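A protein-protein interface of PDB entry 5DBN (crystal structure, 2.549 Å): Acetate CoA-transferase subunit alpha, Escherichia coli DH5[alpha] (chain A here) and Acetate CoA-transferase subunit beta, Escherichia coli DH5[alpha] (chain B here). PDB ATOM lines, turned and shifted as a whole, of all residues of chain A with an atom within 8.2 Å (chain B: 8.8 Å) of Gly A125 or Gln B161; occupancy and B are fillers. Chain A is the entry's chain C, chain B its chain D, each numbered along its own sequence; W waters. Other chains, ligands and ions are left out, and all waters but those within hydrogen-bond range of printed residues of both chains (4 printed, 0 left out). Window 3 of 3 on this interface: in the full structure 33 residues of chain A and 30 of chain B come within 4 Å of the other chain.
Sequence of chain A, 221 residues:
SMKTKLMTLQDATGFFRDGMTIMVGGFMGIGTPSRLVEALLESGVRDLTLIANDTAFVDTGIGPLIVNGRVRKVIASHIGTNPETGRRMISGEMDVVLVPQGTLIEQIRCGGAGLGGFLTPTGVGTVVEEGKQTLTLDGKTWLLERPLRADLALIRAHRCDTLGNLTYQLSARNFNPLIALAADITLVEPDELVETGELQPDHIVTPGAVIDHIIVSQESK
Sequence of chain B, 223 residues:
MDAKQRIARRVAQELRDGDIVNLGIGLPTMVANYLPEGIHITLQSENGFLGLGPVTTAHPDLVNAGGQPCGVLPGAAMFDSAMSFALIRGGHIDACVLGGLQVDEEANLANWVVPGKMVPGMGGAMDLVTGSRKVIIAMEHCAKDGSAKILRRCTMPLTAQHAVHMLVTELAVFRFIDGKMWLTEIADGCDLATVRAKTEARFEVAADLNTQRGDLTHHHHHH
OG1 of Thr A122 is in hydrogen-bond range of OG1 of Thr B130.
O of Met B126 lies within hydrogen-bond range of OG1 of Thr B130 (2.6 Å). O of Leu B109 lies within hydrogen-bond range of N of Thr B159. O of Gly A123 is in hydrogen-bond range of OG1 of Thr A126. The backbone NH (N) of Gly A125 lies within hydrogen-bond range of the side-chain carboxylate (OE1) of Glu A129, at 2.9 Å. OG1 of Thr A126 sits close to N of Val A128. The indole nitrogen (NE1) of Trp B112 sits at hydrogen-bond distance from the backbone carbonyl oxygen (O) of Leu B158 (3.2 Å).
Thr A122 touches Met B126 (CG2 to CB, 3.3 Å). Val A124 touches Gln B161 (CG1 to NE2, 3.6 Å). Gly A125 touches Leu B158. Gly A125 touches Gln B161. O of Leu B158 touches CG2 of Thr A126, at 3.5 Å. O of Thr B159 touches CG2 of Thr A126, at 3.6 Å. CG2 of Val A128 touches CE of Met B126 (3.8 Å).
Of chain B, only Leu B158 and Gln B161 come within 4 Å of Gly A125. Gln B161 touches two residues of chain A. Val A124 touches one residue of chain B. Of the printed residues of chain B, Thr A126 touches Leu B158 (3.5 Å) and Thr B159 (3.6 Å). Printed residues of chain B within 4 Å of Val A128: Met B126 (3.8 Å). Printed residues of chain A within 4 Å of Met B126: Thr A122 and Val A128. Of the printed residues of chain A, Thr B159 touches Thr A126. Printed residues of chain A within 4 Å of Leu B158: Gly A125 (3.8 Å) and Thr A126 (3.5 Å). Of the printed residues of chain A, Thr B130 touches Thr A122. The nearest printed residue of chain B that does not touch Thr A122 is Thr B159 (6.3 Å).
Water W3 lies within hydrogen-bond range of O of Val A124 (2.5 Å) and N of Gln B161 (3.3 Å). Water W4 lies within hydrogen-bond range of O of Thr B159 (2.7 Å), N of Gly A123 (2.9 Å) and SD of Met B126 (3.8 Å). Water W1 bridges the backbone carbonyl oxygen (O) of Gly A125 (2.8 Å) and the side-chain amide oxygen (OE1) of Gln B161 (3.5 Å). Water W2 bridges O of Leu B158 (3.0 Å) and N of Val A127 (3.2 Å).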
ATOM      1  N   PRO A 121      14.279 -25.647 -24.401  1.00  0.00           N
ATOM      2  CA  PRO A 121      15.040 -24.568 -25.038  1.00  0.00           C
ATOM      3  C   PRO A 121      14.787 -23.212 -24.396  1.00  0.00           C
ATOM      4  O   PRO A 121      15.504 -22.251 -24.667  1.00  0.00           O
ATOM      5  CB  PRO A 121      14.520 -24.584 -26.470  1.00  0.00           C
ATOM      6  CG  PRO A 121      13.118 -25.047 -26.349  1.00  0.00           C
ATOM      7  CD  PRO A 121      13.068 -25.984 -25.171  1.00  0.00           C
ATOM      8  N   THR A 122      13.763 -23.145 -23.553  1.00  0.00           N
ATOM      9  CA  THR A 122      13.412 -21.906 -22.875  1.00  0.00           C
ATOM     10  C   THR A 122      14.473 -21.528 -21.851  1.00  0.00           C
ATOM     11  O   THR A 122      14.821 -22.321 -20.977  1.00  0.00           O
ATOM     12  CB  THR A 122      12.041 -22.027 -22.182  1.00  0.00           C
ATOM     13  OG1 THR A 122      11.062 -22.454 -23.136  1.00  0.00           O
ATOM     14  CG2 THR A 122      11.614 -20.696 -21.582  1.00  0.00           C
ATOM     15  N   GLY A 123      14.987 -20.310 -21.977  1.00  0.00           N
ATOM     16  CA  GLY A 123      15.939 -19.774 -21.023  1.00  0.00           C
ATOM     17  C   GLY A 123      17.382 -19.916 -21.465  1.00  0.00           C
ATOM     18  O   GLY A 123      18.284 -19.400 -20.808  1.00  0.00           O
ATOM     19  N   VAL A 124      17.609 -20.616 -22.572  1.00  0.00           N
ATOM     20  CA  VAL A 124      18.957 -20.754 -23.107  1.00  0.00           C
ATOM     21  C   VAL A 124      19.472 -19.383 -23.525  1.00  0.00           C
ATOM     22  O   VAL A 124      18.786 -18.643 -24.228  1.00  0.00           O
ATOM     23  CB  VAL A 124      19.008 -21.724 -24.307  1.00  0.00           C
ATOM     24  CG1 VAL A 124      20.412 -21.776 -24.905  1.00  0.00           C
ATOM     25  CG2 VAL A 124      18.565 -23.115 -23.884  1.00  0.00           C
ATOM     26  N   GLY A 125      20.677 -19.049 -23.079  1.00  0.00           N
ATOM     27  CA  GLY A 125      21.294 -17.779 -23.423  1.00  0.00           C
ATOM     28  C   GLY A 125      20.828 -16.631 -22.545  1.00  0.00           C
ATOM     29  O   GLY A 125      21.145 -15.472 -22.820  1.00  0.00           O
ATOM     30  N   THR A 126      20.082 -16.953 -21.490  1.00  0.00           N
ATOM     31  CA  THR A 126      19.576 -15.947 -20.559  1.00  0.00           C
ATOM     32  C   THR A 126      20.104 -16.218 -19.154  1.00  0.00           C
ATOM     33  O   THR A 126      20.878 -17.152 -18.944  1.00  0.00           O
ATOM     34  CB  THR A 126      18.035 -15.929 -20.526  1.00  0.00           C
ATOM     35  OG1 THR A 126      17.548 -17.087 -19.839  1.00  0.00           O
ATOM     36  CG2 THR A 126      17.466 -15.890 -21.938  1.00  0.00           C
ATOM     37  N   VAL A 127      19.694 -15.390 -18.196  1.00  0.00           N
ATOM     38  CA  VAL A 127      20.104 -15.563 -16.805  1.00  0.00           C
ATOM     39  C   VAL A 127      19.497 -16.825 -16.188  1.00  0.00           C
ATOM     40  O   VAL A 127      19.971 -17.312 -15.161  1.00  0.00           O
ATOM     41  CB  VAL A 127      19.708 -14.347 -15.943  1.00  0.00           C
ATOM     42  CG1 VAL A 127      20.475 -13.110 -16.388  1.00  0.00           C
ATOM     43  CG2 VAL A 127      18.198 -14.103 -16.001  1.00  0.00           C
ATOM     44  N   VAL A 128      18.447 -17.345 -16.816  1.00  0.00           N
ATOM     45  CA  VAL A 128      17.800 -18.568 -16.352  1.00  0.00           C
ATOM     46  C   VAL A 128      18.764 -19.742 -16.488  1.00  0.00           C
ATOM     47  O   VAL A 128      18.703 -20.707 -15.726  1.00  0.00           O
ATOM     48  CB  VAL A 128      16.501 -18.852 -17.142  1.00  0.00           C
ATOM     49  CG1 VAL A 128      15.857 -20.158 -16.694  1.00  0.00           C
ATOM     50  CG2 VAL A 128      15.522 -17.693 -16.991  1.00  0.00           C
ATOM     51  N   GLU A 129      19.665 -19.629 -17.456  1.00  0.00           N
ATOM     52  CA  GLU A 129      20.643 -20.669 -17.749  1.00  0.00           C
ATOM     53  C   GLU A 129      21.677 -20.807 -16.632  1.00  0.00           C
ATOM     54  O   GLU A 129      22.341 -21.839 -16.513  1.00  0.00           O
ATOM     55  CB  GLU A 129      21.336 -20.356 -19.077  1.00  0.00           C
ATOM     56  CG  GLU A 129      22.370 -21.369 -19.523  1.00  0.00           C
ATOM     57  CD  GLU A 129      22.896 -21.063 -20.910  1.00  0.00           C
ATOM     58  OE1 GLU A 129      22.872 -19.879 -21.304  1.00  0.00           O
ATOM     59  OE2 GLU A 129      23.320 -22.002 -21.612  1.00  0.00           O
ATOM     60  N   GLU A 130      21.814 -19.765 -15.819  1.00  0.00           N
ATOM     61  CA  GLU A 130      22.828 -19.732 -14.769  1.00  0.00           C
ATOM     62  C   GLU A 130      22.665 -20.872 -13.763  1.00  0.00           C
ATOM     63  O   GLU A 130      21.580 -21.089 -13.221  1.00  0.00           O
ATOM     64  CB  GLU A 130      22.782 -18.389 -14.038  1.00  0.00           C
ATOM     65  N   THR A 134      23.612 -27.723 -19.366  1.00  0.00           N
ATOM     66  CA  THR A 134      23.165 -27.575 -20.742  1.00  0.00           C
ATOM     67  C   THR A 134      23.625 -28.774 -21.563  1.00  0.00           C
ATOM     68  O   THR A 134      24.763 -29.224 -21.436  1.00  0.00           O
ATOM     69  CB  THR A 134      23.706 -26.286 -21.377  1.00  0.00           C
ATOM     70  OG1 THR A 134      25.125 -26.391 -21.543  1.00  0.00           O
ATOM     71  CG2 THR A 134      23.384 -25.088 -20.505  1.00  0.00           C
ATOM     72  N   THR A 141      20.944 -26.558 -28.368  1.00  0.00           N
ATOM     73  CA  THR A 141      21.276 -26.520 -26.948  1.00  0.00           C
ATOM     74  C   THR A 141      20.005 -26.512 -26.103  1.00  0.00           C
ATOM     75  O   THR A 141      19.068 -25.767 -26.386  1.00  0.00           O
ATOM     76  CB  THR A 141      22.127 -25.279 -26.602  1.00  0.00           C
ATOM     77  OG1 THR A 141      23.338 -25.299 -27.368  1.00  0.00           O
ATOM     78  CG2 THR A 141      22.471 -25.246 -25.114  1.00  0.00           C
ATOM     79  N   LEU A 143      18.413 -26.562 -21.940  1.00  0.00           N
ATOM     80  CA  LEU A 143      18.588 -26.509 -20.494  1.00  0.00           C
ATOM     81  C   LEU A 143      17.996 -27.759 -19.855  1.00  0.00           C
ATOM     82  O   LEU A 143      16.850 -28.120 -20.130  1.00  0.00           O
ATOM     83  CB  LEU A 143      17.925 -25.267 -19.897  1.00  0.00           C
ATOM     84  CG  LEU A 143      18.364 -23.896 -20.408  1.00  0.00           C
ATOM     85  CD1 LEU A 143      17.817 -22.814 -19.497  1.00  0.00           C
ATOM     86  CD2 LEU A 143      19.880 -23.799 -20.502  1.00  0.00           C
ATOM     87  N   ASP B 104      18.027  -6.754 -31.473  1.00  0.00           N
ATOM     88  CA  ASP B 104      19.280  -6.525 -32.193  1.00  0.00           C
ATOM     89  C   ASP B 104      19.429  -7.367 -33.460  1.00  0.00           C
ATOM     90  O   ASP B 104      18.592  -8.217 -33.765  1.00  0.00           O
ATOM     91  CB  ASP B 104      20.477  -6.769 -31.264  1.00  0.00           C
ATOM     92  CG  ASP B 104      20.510  -8.176 -30.689  1.00  0.00           C
ATOM     93  OD1 ASP B 104      19.991  -9.116 -31.328  1.00  0.00           O
ATOM     94  OD2 ASP B 104      21.073  -8.340 -29.586  1.00  0.00           O
ATOM     95  N   GLU B 106      21.183  -9.753 -34.212  1.00  0.00           N
ATOM     96  CA  GLU B 106      21.269 -11.194 -33.987  1.00  0.00           C
ATOM     97  C   GLU B 106      19.909 -11.778 -33.601  1.00  0.00           C
ATOM     98  O   GLU B 106      19.826 -12.911 -33.130  1.00  0.00           O
ATOM     99  CB  GLU B 106      22.297 -11.500 -32.894  1.00  0.00           C
ATOM    100  CG  GLU B 106      23.716 -11.045 -33.215  1.00  0.00           C
ATOM    101  CD  GLU B 106      24.310 -11.766 -34.412  1.00  0.00           C
ATOM    102  OE1 GLU B 106      24.020 -12.969 -34.586  1.00  0.00           O
ATOM    103  OE2 GLU B 106      25.071 -11.134 -35.175  1.00  0.00           O
ATOM    104  N   ALA B 107      18.855 -10.991 -33.801  1.00  0.00           N
ATOM    105  CA  ALA B 107      17.481 -11.411 -33.521  1.00  0.00           C
ATOM    106  C   ALA B 107      17.246 -11.724 -32.042  1.00  0.00           C
ATOM    107  O   ALA B 107      16.297 -12.430 -31.698  1.00  0.00           O
ATOM    108  CB  ALA B 107      17.110 -12.620 -34.381  1.00  0.00           C
ATOM    109  N   ASN B 108      18.107 -11.208 -31.169  1.00  0.00           N
ATOM    110  CA  ASN B 108      17.898 -11.341 -29.729  1.00  0.00           C
ATOM    111  C   ASN B 108      16.783 -10.408 -29.258  1.00  0.00           C
ATOM    112  O   ASN B 108      16.501  -9.398 -29.905  1.00  0.00           O
ATOM    113  CB  ASN B 108      19.187 -11.046 -28.957  1.00  0.00           C
ATOM    114  CG  ASN B 108      20.345 -11.925 -29.393  1.00  0.00           C
ATOM    115  OD1 ASN B 108      20.163 -13.098 -29.723  1.00  0.00           O
ATOM    116  ND2 ASN B 108      21.547 -11.362 -29.392  1.00  0.00           N
ATOM    117  N   LEU B 109      16.154 -10.755 -28.136  1.00  0.00           N
ATOM    118  CA  LEU B 109      15.048  -9.973 -27.584  1.00  0.00           C
ATOM    119  C   LEU B 109      15.219  -9.695 -26.095  1.00  0.00           C
ATOM    120  O   LEU B 109      15.689 -10.551 -25.344  1.00  0.00           O
ATOM    121  CB  LEU B 109      13.717 -10.694 -27.806  1.00  0.00           C
ATOM    122  CG  LEU B 109      12.479 -10.014 -27.207  1.00  0.00           C
ATOM    123  CD1 LEU B 109      12.201  -8.683 -27.890  1.00  0.00           C
ATOM    124  CD2 LEU B 109      11.269 -10.929 -27.270  1.00  0.00           C
ATOM    125  N   ALA B 110      14.832  -8.491 -25.684  1.00  0.00           N
ATOM    126  CA  ALA B 110      14.736  -8.135 -24.272  1.00  0.00           C
ATOM    127  C   ALA B 110      13.406  -7.429 -24.033  1.00  0.00           C
ATOM    128  O   ALA B 110      13.148  -6.376 -24.614  1.00  0.00           O
ATOM    129  CB  ALA B 110      15.901  -7.250 -23.858  1.00  0.00           C
ATOM    130  N   TRP B 112      11.328  -8.271 -20.656  1.00  0.00           N
ATOM    131  CA  TRP B 112      10.746  -8.736 -19.397  1.00  0.00           C
ATOM    132  C   TRP B 112      11.323  -8.037 -18.167  1.00  0.00           C
ATOM    133  O   TRP B 112      10.810  -8.206 -17.061  1.00  0.00           O
ATOM    134  CB  TRP B 112      10.932 -10.248 -19.250  1.00  0.00           C
ATOM    135  CG  TRP B 112      12.324 -10.676 -18.907  1.00  0.00           C
ATOM    136  CD1 TRP B 112      13.375 -10.824 -19.764  1.00  0.00           C
ATOM    137  CD2 TRP B 112      12.814 -11.031 -17.607  1.00  0.00           C
ATOM    138  NE1 TRP B 112      14.491 -11.242 -19.078  1.00  0.00           N
ATOM    139  CE2 TRP B 112      14.171 -11.377 -17.753  1.00  0.00           C
ATOM    140  CE3 TRP B 112      12.237 -11.086 -16.335  1.00  0.00           C
ATOM    141  CZ2 TRP B 112      14.961 -11.770 -16.673  1.00  0.00           C
ATOM    142  CZ3 TRP B 112      13.022 -11.477 -15.265  1.00  0.00           C
ATOM    143  CH2 TRP B 112      14.370 -11.815 -15.442  1.00  0.00           C
ATOM    144  N   MET B 126       9.399 -16.118 -22.475  1.00  0.00           N
ATOM    145  CA  MET B 126      10.498 -16.937 -22.975  1.00  0.00           C
ATOM    146  C   MET B 126       9.981 -18.147 -23.754  1.00  0.00           C
ATOM    147  O   MET B 126      10.459 -18.435 -24.847  1.00  0.00           O
ATOM    148  CB  MET B 126      11.393 -17.394 -21.824  1.00  0.00           C
ATOM    149  CG  MET B 126      11.975 -16.249 -21.013  1.00  0.00           C
ATOM    150  SD  MET B 126      13.456 -16.703 -20.085  1.00  0.00           S
ATOM    151  CE  MET B 126      13.829 -15.155 -19.275  1.00  0.00           C
ATOM    152  N   VAL B 129       8.377 -16.867 -27.168  1.00  0.00           N
ATOM    153  CA  VAL B 129       9.298 -16.480 -28.234  1.00  0.00           C
ATOM    154  C   VAL B 129      10.183 -17.643 -28.694  1.00  0.00           C
ATOM    155  O   VAL B 129      10.649 -17.656 -29.834  1.00  0.00           O
ATOM    156  CB  VAL B 129      10.197 -15.295 -27.801  1.00  0.00           C
ATOM    157  CG1 VAL B 129       9.350 -14.069 -27.494  1.00  0.00           C
ATOM    158  CG2 VAL B 129      11.050 -15.664 -26.604  1.00  0.00           C
ATOM    159  N   THR B 130      10.421 -18.610 -27.812  1.00  0.00           N
ATOM    160  CA  THR B 130      11.174 -19.808 -28.181  1.00  0.00           C
ATOM    161  C   THR B 130      10.298 -20.819 -28.920  1.00  0.00           C
ATOM    162  O   THR B 130      10.787 -21.582 -29.753  1.00  0.00           O
ATOM    163  CB  THR B 130      11.806 -20.496 -26.947  1.00  0.00           C
ATOM    164  OG1 THR B 130      10.808 -20.722 -25.946  1.00  0.00           O
ATOM    165  CG2 THR B 130      12.928 -19.639 -26.365  1.00  0.00           C
ATOM    166  N   ARG B 153      23.659  -4.952 -30.329  1.00  0.00           N
ATOM    167  CA  ARG B 153      23.566  -6.000 -29.319  1.00  0.00           C
ATOM    168  C   ARG B 153      22.782  -5.490 -28.116  1.00  0.00           C
ATOM    169  O   ARG B 153      23.072  -4.416 -27.588  1.00  0.00           O
ATOM    170  CB  ARG B 153      24.961  -6.466 -28.894  1.00  0.00           C
ATOM    171  CG  ARG B 153      24.977  -7.504 -27.773  1.00  0.00           C
ATOM    172  CD  ARG B 153      24.182  -8.751 -28.135  1.00  0.00           C
ATOM    173  NE  ARG B 153      24.390  -9.836 -27.175  1.00  0.00           N
ATOM    174  CZ  ARG B 153      23.709  -9.987 -26.041  1.00  0.00           C
ATOM    175  NH1 ARG B 153      22.768  -9.119 -25.695  1.00  0.00           N
ATOM    176  NH2 ARG B 153      23.977 -11.010 -25.241  1.00  0.00           N
ATOM    177  N   CYS B 154      21.783  -6.260 -27.692  1.00  0.00           N
ATOM    178  CA  CYS B 154      20.972  -5.892 -26.538  1.00  0.00           C
ATOM    179  C   CYS B 154      21.836  -5.736 -25.293  1.00  0.00           C
ATOM    180  O   CYS B 154      22.725  -6.548 -25.036  1.00  0.00           O
ATOM    181  CB  CYS B 154      19.883  -6.938 -26.289  1.00  0.00           C
ATOM    182  SG  CYS B 154      18.606  -7.024 -27.570  1.00  0.00           S
ATOM    183  N   MET B 156      20.156  -4.966 -22.242  1.00  0.00           N
ATOM    184  CA  MET B 156      19.273  -5.415 -21.170  1.00  0.00           C
ATOM    185  C   MET B 156      19.193  -6.937 -21.159  1.00  0.00           C
ATOM    186  O   MET B 156      19.516  -7.581 -22.158  1.00  0.00           O
ATOM    187  CB  MET B 156      17.877  -4.811 -21.329  1.00  0.00           C
ATOM    188  CG  MET B 156      17.857  -3.292 -21.331  1.00  0.00           C
ATOM    189  SD  MET B 156      16.188  -2.619 -21.454  1.00  0.00           S
ATOM    190  CE  MET B 156      16.540  -0.866 -21.540  1.00  0.00           C
ATOM    191  N   PRO B 157      18.766  -7.520 -20.023  1.00  0.00           N
ATOM    192  CA  PRO B 157      18.659  -8.981 -19.921  1.00  0.00           C
ATOM    193  C   PRO B 157      17.767  -9.573 -21.002  1.00  0.00           C
ATOM    194  O   PRO B 157      16.637  -9.122 -21.192  1.00  0.00           O
ATOM    195  CB  PRO B 157      18.047  -9.194 -18.534  1.00  0.00           C
ATOM    196  CG  PRO B 157      18.417  -7.978 -17.768  1.00  0.00           C
ATOM    197  CD  PRO B 157      18.404  -6.856 -18.759  1.00  0.00           C
ATOM    198  N   LEU B 158      18.278 -10.583 -21.698  1.00  0.00           N
ATOM    199  CA  LEU B 158      17.567 -11.168 -22.825  1.00  0.00           C
ATOM    200  C   LEU B 158      16.342 -11.958 -22.389  1.00  0.00           C
ATOM    201  O   LEU B 158      16.345 -12.609 -21.344  1.00  0.00           O
ATOM    202  CB  LEU B 158      18.497 -12.078 -23.632  1.00  0.00           C
ATOM    203  CG  LEU B 158      19.743 -11.445 -24.257  1.00  0.00           C
ATOM    204  CD1 LEU B 158      20.508 -12.484 -25.064  1.00  0.00           C
ATOM    205  CD2 LEU B 158      19.393 -10.250 -25.129  1.00  0.00           C
ATOM    206  N   THR B 159      15.297 -11.888 -23.207  1.00  0.00           N
ATOM    207  CA  THR B 159      14.151 -12.777 -23.084  1.00  0.00           C
ATOM    208  C   THR B 159      14.504 -14.092 -23.763  1.00  0.00           C
ATOM    209  O   THR B 159      14.158 -15.171 -23.283  1.00  0.00           O
ATOM    210  CB  THR B 159      12.888 -12.175 -23.732  1.00  0.00           C
ATOM    211  OG1 THR B 159      12.582 -10.919 -23.114  1.00  0.00           O
ATOM    212  CG2 THR B 159      11.698 -13.118 -23.595  1.00  0.00           C
ATOM    213  N   ALA B 160      15.200 -13.976 -24.890  1.00  0.00           N
ATOM    214  CA  ALA B 160      15.685 -15.127 -25.640  1.00  0.00           C
ATOM    215  C   ALA B 160      16.735 -14.672 -26.646  1.00  0.00           C
ATOM    216  O   ALA B 160      16.885 -13.475 -26.897  1.00  0.00           O
ATOM    217  CB  ALA B 160      14.543 -15.829 -26.345  1.00  0.00           C
ATOM    218  N   GLN B 161      17.456 -15.630 -27.220  1.00  0.00           N
ATOM    219  CA  GLN B 161      18.464 -15.336 -28.230  1.00  0.00           C
ATOM    220  C   GLN B 161      18.054 -15.916 -29.580  1.00  0.00           C
ATOM    221  O   GLN B 161      17.531 -17.028 -29.652  1.00  0.00           O
ATOM    222  CB  GLN B 161      19.828 -15.887 -27.807  1.00  0.00           C
ATOM    223  CG  GLN B 161      19.856 -17.391 -27.581  1.00  0.00           C
ATOM    224  CD  GLN B 161      21.234 -17.896 -27.204  1.00  0.00           C
ATOM    225  OE1 GLN B 161      22.148 -17.111 -26.945  1.00  0.00           O
ATOM    226  NE2 GLN B 161      21.394 -19.214 -27.175  1.00  0.00           N
ATOM    227  N   HIS B 162      18.278 -15.144 -30.641  1.00  0.00           N
ATOM    228  CA  HIS B 162      18.033 -15.601 -32.007  1.00  0.00           C
ATOM    229  C   HIS B 162      16.600 -16.098 -32.204  1.00  0.00           C
ATOM    230  O   HIS B 162      16.380 -17.130 -32.838  1.00  0.00           O
ATOM    231  CB  HIS B 162      19.017 -16.717 -32.369  1.00  0.00           C
ATOM    232  CG  HIS B 162      20.421 -16.455 -31.917  1.00  0.00           C
ATOM    233  ND1 HIS B 162      21.189 -15.429 -32.419  1.00  0.00           N
ATOM    234  CD2 HIS B 162      21.195 -17.088 -31.001  1.00  0.00           C
ATOM    235  CE1 HIS B 162      22.376 -15.441 -31.839  1.00  0.00           C
ATOM    236  NE2 HIS B 162      22.403 -16.440 -30.973  1.00  0.00           N
ATOM    237  N   ALA B 163      15.635 -15.360 -31.658  1.00  0.00           N
ATOM    238  CA  ALA B 163      14.244 -15.809 -31.628  1.00  0.00           C
ATOM    239  C   ALA B 163      13.310 -14.959 -32.492  1.00  0.00           C
ATOM    240  O   ALA B 163      12.263 -15.442 -32.928  1.00  0.00           O
ATOM    241  CB  ALA B 163      13.742 -15.823 -30.192  1.00  0.00           C
ATOM    242  N   VAL B 164      13.684 -13.707 -32.745  1.00  0.00           N
ATOM    243  CA  VAL B 164      12.802 -12.785 -33.461  1.00  0.00           C
ATOM    244  C   VAL B 164      12.799 -13.068 -34.959  1.00  0.00           C
ATOM    245  O   VAL B 164      13.855 -13.202 -35.577  1.00  0.00           O
ATOM    246  CB  VAL B 164      13.205 -11.313 -33.228  1.00  0.00           C
ATOM    247  CG1 VAL B 164      12.240 -10.371 -33.941  1.00  0.00           C
ATOM    248  CG2 VAL B 164      13.242 -10.997 -31.745  1.00  0.00           C
HETATM  249  O   HOH W   1      23.303 -14.922 -24.513  1.00  0.00           O
HETATM  250  O   HOH W   2      18.532 -12.650 -19.271  1.00  0.00           O
HETATM  251  O   HOH W   3      16.660 -18.337 -25.568  1.00  0.00           O
HETATM  252  O   HOH W   4      14.729 -17.818 -23.469  1.00  0.00           O
